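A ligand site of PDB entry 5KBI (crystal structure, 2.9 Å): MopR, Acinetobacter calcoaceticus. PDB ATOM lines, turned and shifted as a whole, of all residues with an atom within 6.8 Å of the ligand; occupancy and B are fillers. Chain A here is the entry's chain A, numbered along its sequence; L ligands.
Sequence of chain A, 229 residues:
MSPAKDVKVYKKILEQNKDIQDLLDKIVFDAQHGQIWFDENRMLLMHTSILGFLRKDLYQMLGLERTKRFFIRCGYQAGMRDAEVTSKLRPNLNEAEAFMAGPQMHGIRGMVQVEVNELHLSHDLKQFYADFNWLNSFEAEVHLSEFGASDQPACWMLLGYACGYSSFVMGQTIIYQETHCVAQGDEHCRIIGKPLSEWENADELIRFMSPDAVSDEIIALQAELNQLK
O1 of the ligand is in hydrogen-bond range of ND1 of His 106 (2.6 Å).
The indole nitrogen of Trp 134 lies within hydrogen-bond range of an oxygen (O2) of the ligand (3.1 Å).
N of Val 112 is in hydrogen-bond range of O of His 106, at 3.2 Å.
O of Phe 132 is in hydrogen-bond range of N of Ile 191 (3.1 Å).
The side-chain hydroxyl (OH) of Tyr 165 lies within hydrogen-bond range of the backbone NH (N) of Gly 102.
The backbone carbonyl oxygen (O) of Phe 99 sits at hydrogen-bond distance from the side-chain hydroxyl (OH) of Tyr 165, 2.9 Å away.
The side-chain hydroxyl (OH) of Tyr 176 is in hydrogen-bond range of the side-chain hydroxyl (OG) of Ser 166, at 2.7 Å.
N of Tyr 176 sits at hydrogen-bond distance from SG of Cys 163, 3.4 Å away.
The backbone carbonyl oxygen (O) of Ala 162 lies within hydrogen-bond range of the side-chain hydroxyl (OG) of Ser 166 (2.9 Å).
CZ of Phe 99 touches C6 of the ligand, 3.8 Å away.
Gly 102 touches the ligand.
CD of Pro 103 touches C1 of the ligand (3.4 Å).
CG2 of Val 114 touches O1 of the ligand, 3.3 Å away.
CD2 of Phe 132 touches O2 of the ligand (3.4 Å).
Tyr 161 touches the ligand (CE1 to C2, 3.7 Å).
Tyr 165 touches the ligand (CD2 to C1, 3.6 Å).
Ser 166 touches the ligand.
OH of Tyr 176 touches C5 of the ligand (3.7 Å).
Ile 191 touches the ligand (CD1 to O2, 3.4 Å).
The nearest printed residue that does not touch the ligand is Ala 162 (4.2 Å).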
ATOM      1  N   PHE A  99     -23.961  15.774  13.343  1.00  0.00           N
ATOM      2  CA  PHE A  99     -24.470  16.195  12.025  1.00  0.00           C
ATOM      3  C   PHE A  99     -23.786  15.547  10.829  1.00  0.00           C
ATOM      4  O   PHE A  99     -24.415  15.145   9.850  1.00  0.00           O
ATOM      5  CB  PHE A  99     -24.295  17.699  11.850  1.00  0.00           C
ATOM      6  CG  PHE A  99     -24.885  18.192  10.588  1.00  0.00           C
ATOM      7  CD1 PHE A  99     -26.239  18.416  10.501  1.00  0.00           C
ATOM      8  CD2 PHE A  99     -24.090  18.385   9.465  1.00  0.00           C
ATOM      9  CE1 PHE A  99     -26.779  18.873   9.317  1.00  0.00           C
ATOM     10  CE2 PHE A  99     -24.611  18.828   8.276  1.00  0.00           C
ATOM     11  CZ  PHE A  99     -25.972  19.071   8.201  1.00  0.00           C
ATOM     12  N   MET A 100     -22.482  15.512  10.905  1.00  0.00           N
ATOM     13  CA  MET A 100     -21.725  14.897   9.864  1.00  0.00           C
ATOM     14  C   MET A 100     -22.268  13.536   9.393  1.00  0.00           C
ATOM     15  O   MET A 100     -22.219  13.235   8.210  1.00  0.00           O
ATOM     16  CB  MET A 100     -20.249  14.857  10.291  1.00  0.00           C
ATOM     17  CG  MET A 100     -19.590  16.195   9.988  1.00  0.00           C
ATOM     18  SD  MET A 100     -19.844  16.634   8.229  1.00  0.00           S
ATOM     19  CE  MET A 100     -21.318  17.617   8.317  1.00  0.00           C
ATOM     20  N   ALA A 101     -22.832  12.756  10.304  1.00  0.00           N
ATOM     21  CA  ALA A 101     -23.376  11.445   9.961  1.00  0.00           C
ATOM     22  C   ALA A 101     -24.076  11.524   8.597  1.00  0.00           C
ATOM     23  O   ALA A 101     -23.874  10.663   7.731  1.00  0.00           O
ATOM     24  CB  ALA A 101     -24.350  10.957  11.051  1.00  0.00           C
ATOM     25  N   GLY A 102     -24.855  12.593   8.442  1.00  0.00           N
ATOM     26  CA  GLY A 102     -25.619  12.860   7.247  1.00  0.00           C
ATOM     27  C   GLY A 102     -24.729  12.772   6.029  1.00  0.00           C
ATOM     28  O   GLY A 102     -24.870  11.845   5.245  1.00  0.00           O
ATOM     29  N   PRO A 103     -23.832  13.751   5.849  1.00  0.00           N
ATOM     30  CA  PRO A 103     -22.928  13.783   4.689  1.00  0.00           C
ATOM     31  C   PRO A 103     -22.135  12.504   4.500  1.00  0.00           C
ATOM     32  O   PRO A 103     -21.839  12.122   3.358  1.00  0.00           O
ATOM     33  CB  PRO A 103     -22.003  14.942   4.996  1.00  0.00           C
ATOM     34  CG  PRO A 103     -22.847  15.831   5.873  1.00  0.00           C
ATOM     35  CD  PRO A 103     -23.959  15.061   6.492  1.00  0.00           C
ATOM     36  N   GLN A 104     -21.836  11.845   5.610  1.00  0.00           N
ATOM     37  CA  GLN A 104     -21.189  10.545   5.566  1.00  0.00           C
ATOM     38  C   GLN A 104     -22.089   9.436   4.973  1.00  0.00           C
ATOM     39  O   GLN A 104     -21.606   8.554   4.248  1.00  0.00           O
ATOM     40  CB  GLN A 104     -20.735  10.162   6.957  1.00  0.00           C
ATOM     41  CG  GLN A 104     -19.422  10.806   7.332  1.00  0.00           C
ATOM     42  CD  GLN A 104     -19.336  11.160   8.806  1.00  0.00           C
ATOM     43  OE1 GLN A 104     -20.187  10.764   9.634  1.00  0.00           O
ATOM     44  NE2 GLN A 104     -18.310  11.951   9.136  1.00  0.00           N
ATOM     45  N   MET A 105     -23.368   9.481   5.301  1.00  0.00           N
ATOM     46  CA  MET A 105     -24.323   8.514   4.796  1.00  0.00           C
ATOM     47  C   MET A 105     -24.531   8.605   3.314  1.00  0.00           C
ATOM     48  O   MET A 105     -24.646   7.617   2.650  1.00  0.00           O
ATOM     49  CB  MET A 105     -25.680   8.660   5.501  1.00  0.00           C
ATOM     50  CG  MET A 105     -25.751   7.918   6.821  1.00  0.00           C
ATOM     51  SD  MET A 105     -25.116   6.238   6.688  1.00  0.00           S
ATOM     52  CE  MET A 105     -26.536   5.350   6.023  1.00  0.00           C
ATOM     53  N   HIS A 106     -24.575   9.808   2.819  1.00  0.00           N
ATOM     54  CA  HIS A 106     -24.570  10.023   1.409  1.00  0.00           C
ATOM     55  C   HIS A 106     -23.395   9.430   0.679  1.00  0.00           C
ATOM     56  O   HIS A 106     -23.503   9.037  -0.473  1.00  0.00           O
ATOM     57  CB  HIS A 106     -24.624  11.513   1.131  1.00  0.00           C
ATOM     58  CG  HIS A 106     -25.943  11.965   0.530  1.00  0.00           C
ATOM     59  ND1 HIS A 106     -26.246  13.255   0.372  1.00  0.00           N
ATOM     60  CD2 HIS A 106     -27.043  11.227   0.082  1.00  0.00           C
ATOM     61  CE1 HIS A 106     -27.465  13.347  -0.195  1.00  0.00           C
ATOM     62  NE2 HIS A 106     -27.961  12.099  -0.346  1.00  0.00           N
ATOM     63  N   GLY A 107     -22.247   9.408   1.337  1.00  0.00           N
ATOM     64  CA  GLY A 107     -21.078   8.716   0.817  1.00  0.00           C
ATOM     65  C   GLY A 107     -21.325   7.227   0.856  1.00  0.00           C
ATOM     66  O   GLY A 107     -21.303   6.571  -0.179  1.00  0.00           O
ATOM     67  N   VAL A 112     -23.171  10.571  -3.256  1.00  0.00           N
ATOM     68  CA  VAL A 112     -22.372  11.770  -3.396  1.00  0.00           C
ATOM     69  C   VAL A 112     -21.301  11.899  -2.308  1.00  0.00           C
ATOM     70  O   VAL A 112     -21.480  11.421  -1.173  1.00  0.00           O
ATOM     71  CB  VAL A 112     -23.264  13.017  -3.415  1.00  0.00           C
ATOM     72  CG1 VAL A 112     -23.608  13.454  -2.000  1.00  0.00           C
ATOM     73  CG2 VAL A 112     -22.567  14.104  -4.212  1.00  0.00           C
ATOM     74  N   GLN A 113     -20.214  12.561  -2.705  1.00  0.00           N
ATOM     75  CA  GLN A 113     -19.111  12.880  -1.834  1.00  0.00           C
ATOM     76  C   GLN A 113     -19.176  14.297  -1.291  1.00  0.00           C
ATOM     77  O   GLN A 113     -19.025  15.288  -2.037  1.00  0.00           O
ATOM     78  CB  GLN A 113     -17.811  12.744  -2.593  1.00  0.00           C
ATOM     79  CG  GLN A 113     -16.707  12.648  -1.583  1.00  0.00           C
ATOM     80  CD  GLN A 113     -15.385  12.996  -2.134  1.00  0.00           C
ATOM     81  OE1 GLN A 113     -14.856  12.329  -3.023  1.00  0.00           O
ATOM     82  NE2 GLN A 113     -14.802  14.041  -1.568  1.00  0.00           N
ATOM     83  N   VAL A 114     -19.410  14.390   0.014  1.00  0.00           N
ATOM     84  CA  VAL A 114     -19.546  15.718   0.602  1.00  0.00           C
ATOM     85  C   VAL A 114     -18.249  16.288   1.144  1.00  0.00           C
ATOM     86  O   VAL A 114     -17.483  15.583   1.745  1.00  0.00           O
ATOM     87  CB  VAL A 114     -20.625  15.722   1.654  1.00  0.00           C
ATOM     88  CG1 VAL A 114     -20.870  17.141   2.138  1.00  0.00           C
ATOM     89  CG2 VAL A 114     -21.873  15.126   1.040  1.00  0.00           C
ATOM     90  N   PHE A 128     -28.085  27.903  11.595  1.00  0.00           N
ATOM     91  CA  PHE A 128     -27.493  26.920  10.733  1.00  0.00           C
ATOM     92  C   PHE A 128     -27.036  27.611   9.472  1.00  0.00           C
ATOM     93  O   PHE A 128     -27.714  28.472   8.919  1.00  0.00           O
ATOM     94  CB  PHE A 128     -28.521  25.819  10.396  1.00  0.00           C
ATOM     95  CG  PHE A 128     -27.939  24.668   9.611  1.00  0.00           C
ATOM     96  CD1 PHE A 128     -27.752  24.761   8.220  1.00  0.00           C
ATOM     97  CD2 PHE A 128     -27.523  23.513  10.250  1.00  0.00           C
ATOM     98  CE1 PHE A 128     -27.187  23.738   7.493  1.00  0.00           C
ATOM     99  CE2 PHE A 128     -26.958  22.490   9.523  1.00  0.00           C
ATOM    100  CZ  PHE A 128     -26.789  22.598   8.139  1.00  0.00           C
ATOM    101  N   ALA A 130     -24.747  26.101   6.095  1.00  0.00           N
ATOM    102  CA  ALA A 130     -23.854  25.128   5.549  1.00  0.00           C
ATOM    103  C   ALA A 130     -23.461  25.466   4.118  1.00  0.00           C
ATOM    104  O   ALA A 130     -24.284  25.865   3.280  1.00  0.00           O
ATOM    105  CB  ALA A 130     -24.480  23.751   5.609  1.00  0.00           C
ATOM    106  N   PHE A 132     -21.249  23.291   1.396  1.00  0.00           N
ATOM    107  CA  PHE A 132     -20.506  22.059   1.009  1.00  0.00           C
ATOM    108  C   PHE A 132     -20.355  21.910  -0.478  1.00  0.00           C
ATOM    109  O   PHE A 132     -21.147  22.430  -1.240  1.00  0.00           O
ATOM    110  CB  PHE A 132     -21.245  20.821   1.460  1.00  0.00           C
ATOM    111  CG  PHE A 132     -21.722  20.876   2.880  1.00  0.00           C
ATOM    112  CD1 PHE A 132     -20.945  21.455   3.881  1.00  0.00           C
ATOM    113  CD2 PHE A 132     -22.925  20.304   3.223  1.00  0.00           C
ATOM    114  CE1 PHE A 132     -21.380  21.488   5.183  1.00  0.00           C
ATOM    115  CE2 PHE A 132     -23.357  20.322   4.535  1.00  0.00           C
ATOM    116  CZ  PHE A 132     -22.588  20.897   5.521  1.00  0.00           C
ATOM    117  N   ASN A 133     -19.305  21.202  -0.896  1.00  0.00           N
ATOM    118  CA  ASN A 133     -19.170  20.780  -2.272  1.00  0.00           C
ATOM    119  C   ASN A 133     -19.656  19.356  -2.382  1.00  0.00           C
ATOM    120  O   ASN A 133     -19.239  18.458  -1.657  1.00  0.00           O
ATOM    121  CB  ASN A 133     -17.689  20.815  -2.746  1.00  0.00           C
ATOM    122  CG  ASN A 133     -17.098  22.221  -2.836  1.00  0.00           C
ATOM    123  OD1 ASN A 133     -17.764  23.214  -3.144  1.00  0.00           O
ATOM    124  ND2 ASN A 133     -15.811  22.294  -2.586  1.00  0.00           N
ATOM    125  N   TRP A 134     -20.541  19.128  -3.336  1.00  0.00           N
ATOM    126  CA  TRP A 134     -20.884  17.774  -3.727  1.00  0.00           C
ATOM    127  C   TRP A 134     -19.965  17.365  -4.822  1.00  0.00           C
ATOM    128  O   TRP A 134     -19.907  18.056  -5.829  1.00  0.00           O
ATOM    129  CB  TRP A 134     -22.279  17.779  -4.268  1.00  0.00           C
ATOM    130  CG  TRP A 134     -23.332  17.654  -3.204  1.00  0.00           C
ATOM    131  CD1 TRP A 134     -23.185  17.195  -1.883  1.00  0.00           C
ATOM    132  CD2 TRP A 134     -24.766  17.930  -3.358  1.00  0.00           C
ATOM    133  NE1 TRP A 134     -24.395  17.198  -1.241  1.00  0.00           N
ATOM    134  CE2 TRP A 134     -25.384  17.626  -2.053  1.00  0.00           C
ATOM    135  CE3 TRP A 134     -25.573  18.393  -4.407  1.00  0.00           C
ATOM    136  CZ2 TRP A 134     -26.737  17.797  -1.832  1.00  0.00           C
ATOM    137  CZ3 TRP A 134     -26.923  18.550  -4.177  1.00  0.00           C
ATOM    138  CH2 TRP A 134     -27.503  18.256  -2.909  1.00  0.00           C
ATOM    139  N   LEU A 158     -30.630  14.228  -3.928  1.00  0.00           N
ATOM    140  CA  LEU A 158     -29.546  14.640  -3.061  1.00  0.00           C
ATOM    141  C   LEU A 158     -29.910  15.899  -2.302  1.00  0.00           C
ATOM    142  O   LEU A 158     -29.556  16.044  -1.126  1.00  0.00           O
ATOM    143  CB  LEU A 158     -28.300  14.909  -3.872  1.00  0.00           C
ATOM    144  CG  LEU A 158     -27.759  13.744  -4.686  1.00  0.00           C
ATOM    145  CD1 LEU A 158     -26.429  14.101  -5.351  1.00  0.00           C
ATOM    146  CD2 LEU A 158     -27.634  12.484  -3.831  1.00  0.00           C
ATOM    147  N   TYR A 161     -32.744  15.219   0.217  1.00  0.00           N
ATOM    148  CA  TYR A 161     -32.161  14.496   1.309  1.00  0.00           C
ATOM    149  C   TYR A 161     -31.434  15.472   2.170  1.00  0.00           C
ATOM    150  O   TYR A 161     -31.569  15.454   3.387  1.00  0.00           O
ATOM    151  CB  TYR A 161     -31.191  13.482   0.755  1.00  0.00           C
ATOM    152  CG  TYR A 161     -30.477  12.632   1.780  1.00  0.00           C
ATOM    153  CD1 TYR A 161     -29.311  13.083   2.381  1.00  0.00           C
ATOM    154  CD2 TYR A 161     -30.940  11.345   2.126  1.00  0.00           C
ATOM    155  CE1 TYR A 161     -28.633  12.306   3.296  1.00  0.00           C
ATOM    156  CE2 TYR A 161     -30.252  10.557   3.031  1.00  0.00           C
ATOM    157  CZ  TYR A 161     -29.114  11.065   3.609  1.00  0.00           C
ATOM    158  OH  TYR A 161     -28.401  10.330   4.533  1.00  0.00           O
ATOM    159  N   ALA A 162     -30.644  16.327   1.536  1.00  0.00           N
ATOM    160  CA  ALA A 162     -29.944  17.389   2.270  1.00  0.00           C
ATOM    161  C   ALA A 162     -30.874  18.159   3.236  1.00  0.00           C
ATOM    162  O   ALA A 162     -30.627  18.235   4.423  1.00  0.00           O
ATOM    163  CB  ALA A 162     -29.271  18.347   1.301  1.00  0.00           C
ATOM    164  N   CYS A 163     -31.954  18.701   2.689  1.00  0.00           N
ATOM    165  CA  CYS A 163     -32.914  19.496   3.440  1.00  0.00           C
ATOM    166  C   CYS A 163     -33.549  18.647   4.518  1.00  0.00           C
ATOM    167  O   CYS A 163     -33.727  19.110   5.633  1.00  0.00           O
ATOM    168  CB  CYS A 163     -33.980  20.087   2.505  1.00  0.00           C
ATOM    169  SG  CYS A 163     -33.331  21.067   1.095  1.00  0.00           S
ATOM    170  N   TYR A 165     -32.472  15.601   6.078  1.00  0.00           N
ATOM    171  CA  TYR A 165     -31.540  15.255   7.120  1.00  0.00           C
ATOM    172  C   TYR A 165     -31.387  16.431   8.080  1.00  0.00           C
ATOM    173  O   TYR A 165     -31.623  16.298   9.271  1.00  0.00           O
ATOM    174  CB  TYR A 165     -30.173  14.851   6.562  1.00  0.00           C
ATOM    175  CG  TYR A 165     -29.176  14.500   7.672  1.00  0.00           C
ATOM    176  CD1 TYR A 165     -29.288  13.289   8.355  1.00  0.00           C
ATOM    177  CD2 TYR A 165     -28.168  15.379   8.053  1.00  0.00           C
ATOM    178  CE1 TYR A 165     -28.425  12.956   9.382  1.00  0.00           C
ATOM    179  CE2 TYR A 165     -27.291  15.060   9.088  1.00  0.00           C
ATOM    180  CZ  TYR A 165     -27.431  13.843   9.747  1.00  0.00           C
ATOM    181  OH  TYR A 165     -26.604  13.476  10.777  1.00  0.00           O
ATOM    182  N   SER A 166     -30.996  17.571   7.519  1.00  0.00           N
ATOM    183  CA  SER A 166     -30.711  18.766   8.274  1.00  0.00           C
ATOM    184  C   SER A 166     -31.880  19.192   9.099  1.00  0.00           C
ATOM    185  O   SER A 166     -31.722  19.445  10.280  1.00  0.00           O
ATOM    186  CB  SER A 166     -30.354  19.876   7.314  1.00  0.00           C
ATOM    187  OG  SER A 166     -29.163  19.514   6.627  1.00  0.00           O
ATOM    188  N   TYR A 176     -31.792  24.043   1.202  1.00  0.00           N
ATOM    189  CA  TYR A 176     -30.544  24.227   0.388  1.00  0.00           C
ATOM    190  C   TYR A 176     -30.739  24.738  -1.031  1.00  0.00           C
ATOM    191  O   TYR A 176     -31.687  24.385  -1.704  1.00  0.00           O
ATOM    192  CB  TYR A 176     -29.756  22.940   0.272  1.00  0.00           C
ATOM    193  CG  TYR A 176     -29.163  22.449   1.559  1.00  0.00           C
ATOM    194  CD1 TYR A 176     -29.975  21.905   2.573  1.00  0.00           C
ATOM    195  CD2 TYR A 176     -27.774  22.501   1.781  1.00  0.00           C
ATOM    196  CE1 TYR A 176     -29.421  21.439   3.772  1.00  0.00           C
ATOM    197  CE2 TYR A 176     -27.236  22.059   2.988  1.00  0.00           C
ATOM    198  CZ  TYR A 176     -28.077  21.531   3.972  1.00  0.00           C
ATOM    199  OH  TYR A 176     -27.541  21.071   5.132  1.00  0.00           O
ATOM    200  N   ILE A 191     -23.697  23.261  -2.888  1.00  0.00           N
ATOM    201  CA  ILE A 191     -24.903  23.687  -2.186  1.00  0.00           C
ATOM    202  C   ILE A 191     -24.647  24.605  -1.020  1.00  0.00           C
ATOM    203  O   ILE A 191     -23.521  24.648  -0.458  1.00  0.00           O
ATOM    204  CB  ILE A 191     -25.703  22.508  -1.652  1.00  0.00           C
ATOM    205  CG1 ILE A 191     -24.796  21.522  -0.953  1.00  0.00           C
ATOM    206  CG2 ILE A 191     -26.432  21.822  -2.782  1.00  0.00           C
ATOM    207  CD1 ILE A 191     -25.399  20.956   0.314  1.00  0.00           C
HETATM  208  C1  LIG L   1     -26.727  15.867   4.765  1.00  0.00           C
HETATM  209  C2  LIG L   1     -26.298  15.213   3.620  1.00  0.00           C
HETATM  210  C3  LIG L   1     -25.645  15.939   2.616  1.00  0.00           C
HETATM  211  O1  LIG L   1     -25.174  15.399   1.441  1.00  0.00           O
HETATM  212  C4  LIG L   1     -25.464  17.292   2.790  1.00  0.00           C
HETATM  213  O2  LIG L   1     -24.813  17.906   1.767  1.00  0.00           O
HETATM  214  C5  LIG L   1     -25.909  17.986   3.924  1.00  0.00           C
HETATM  215  C6  LIG L   1     -26.536  17.248   4.904  1.00  0.00           C
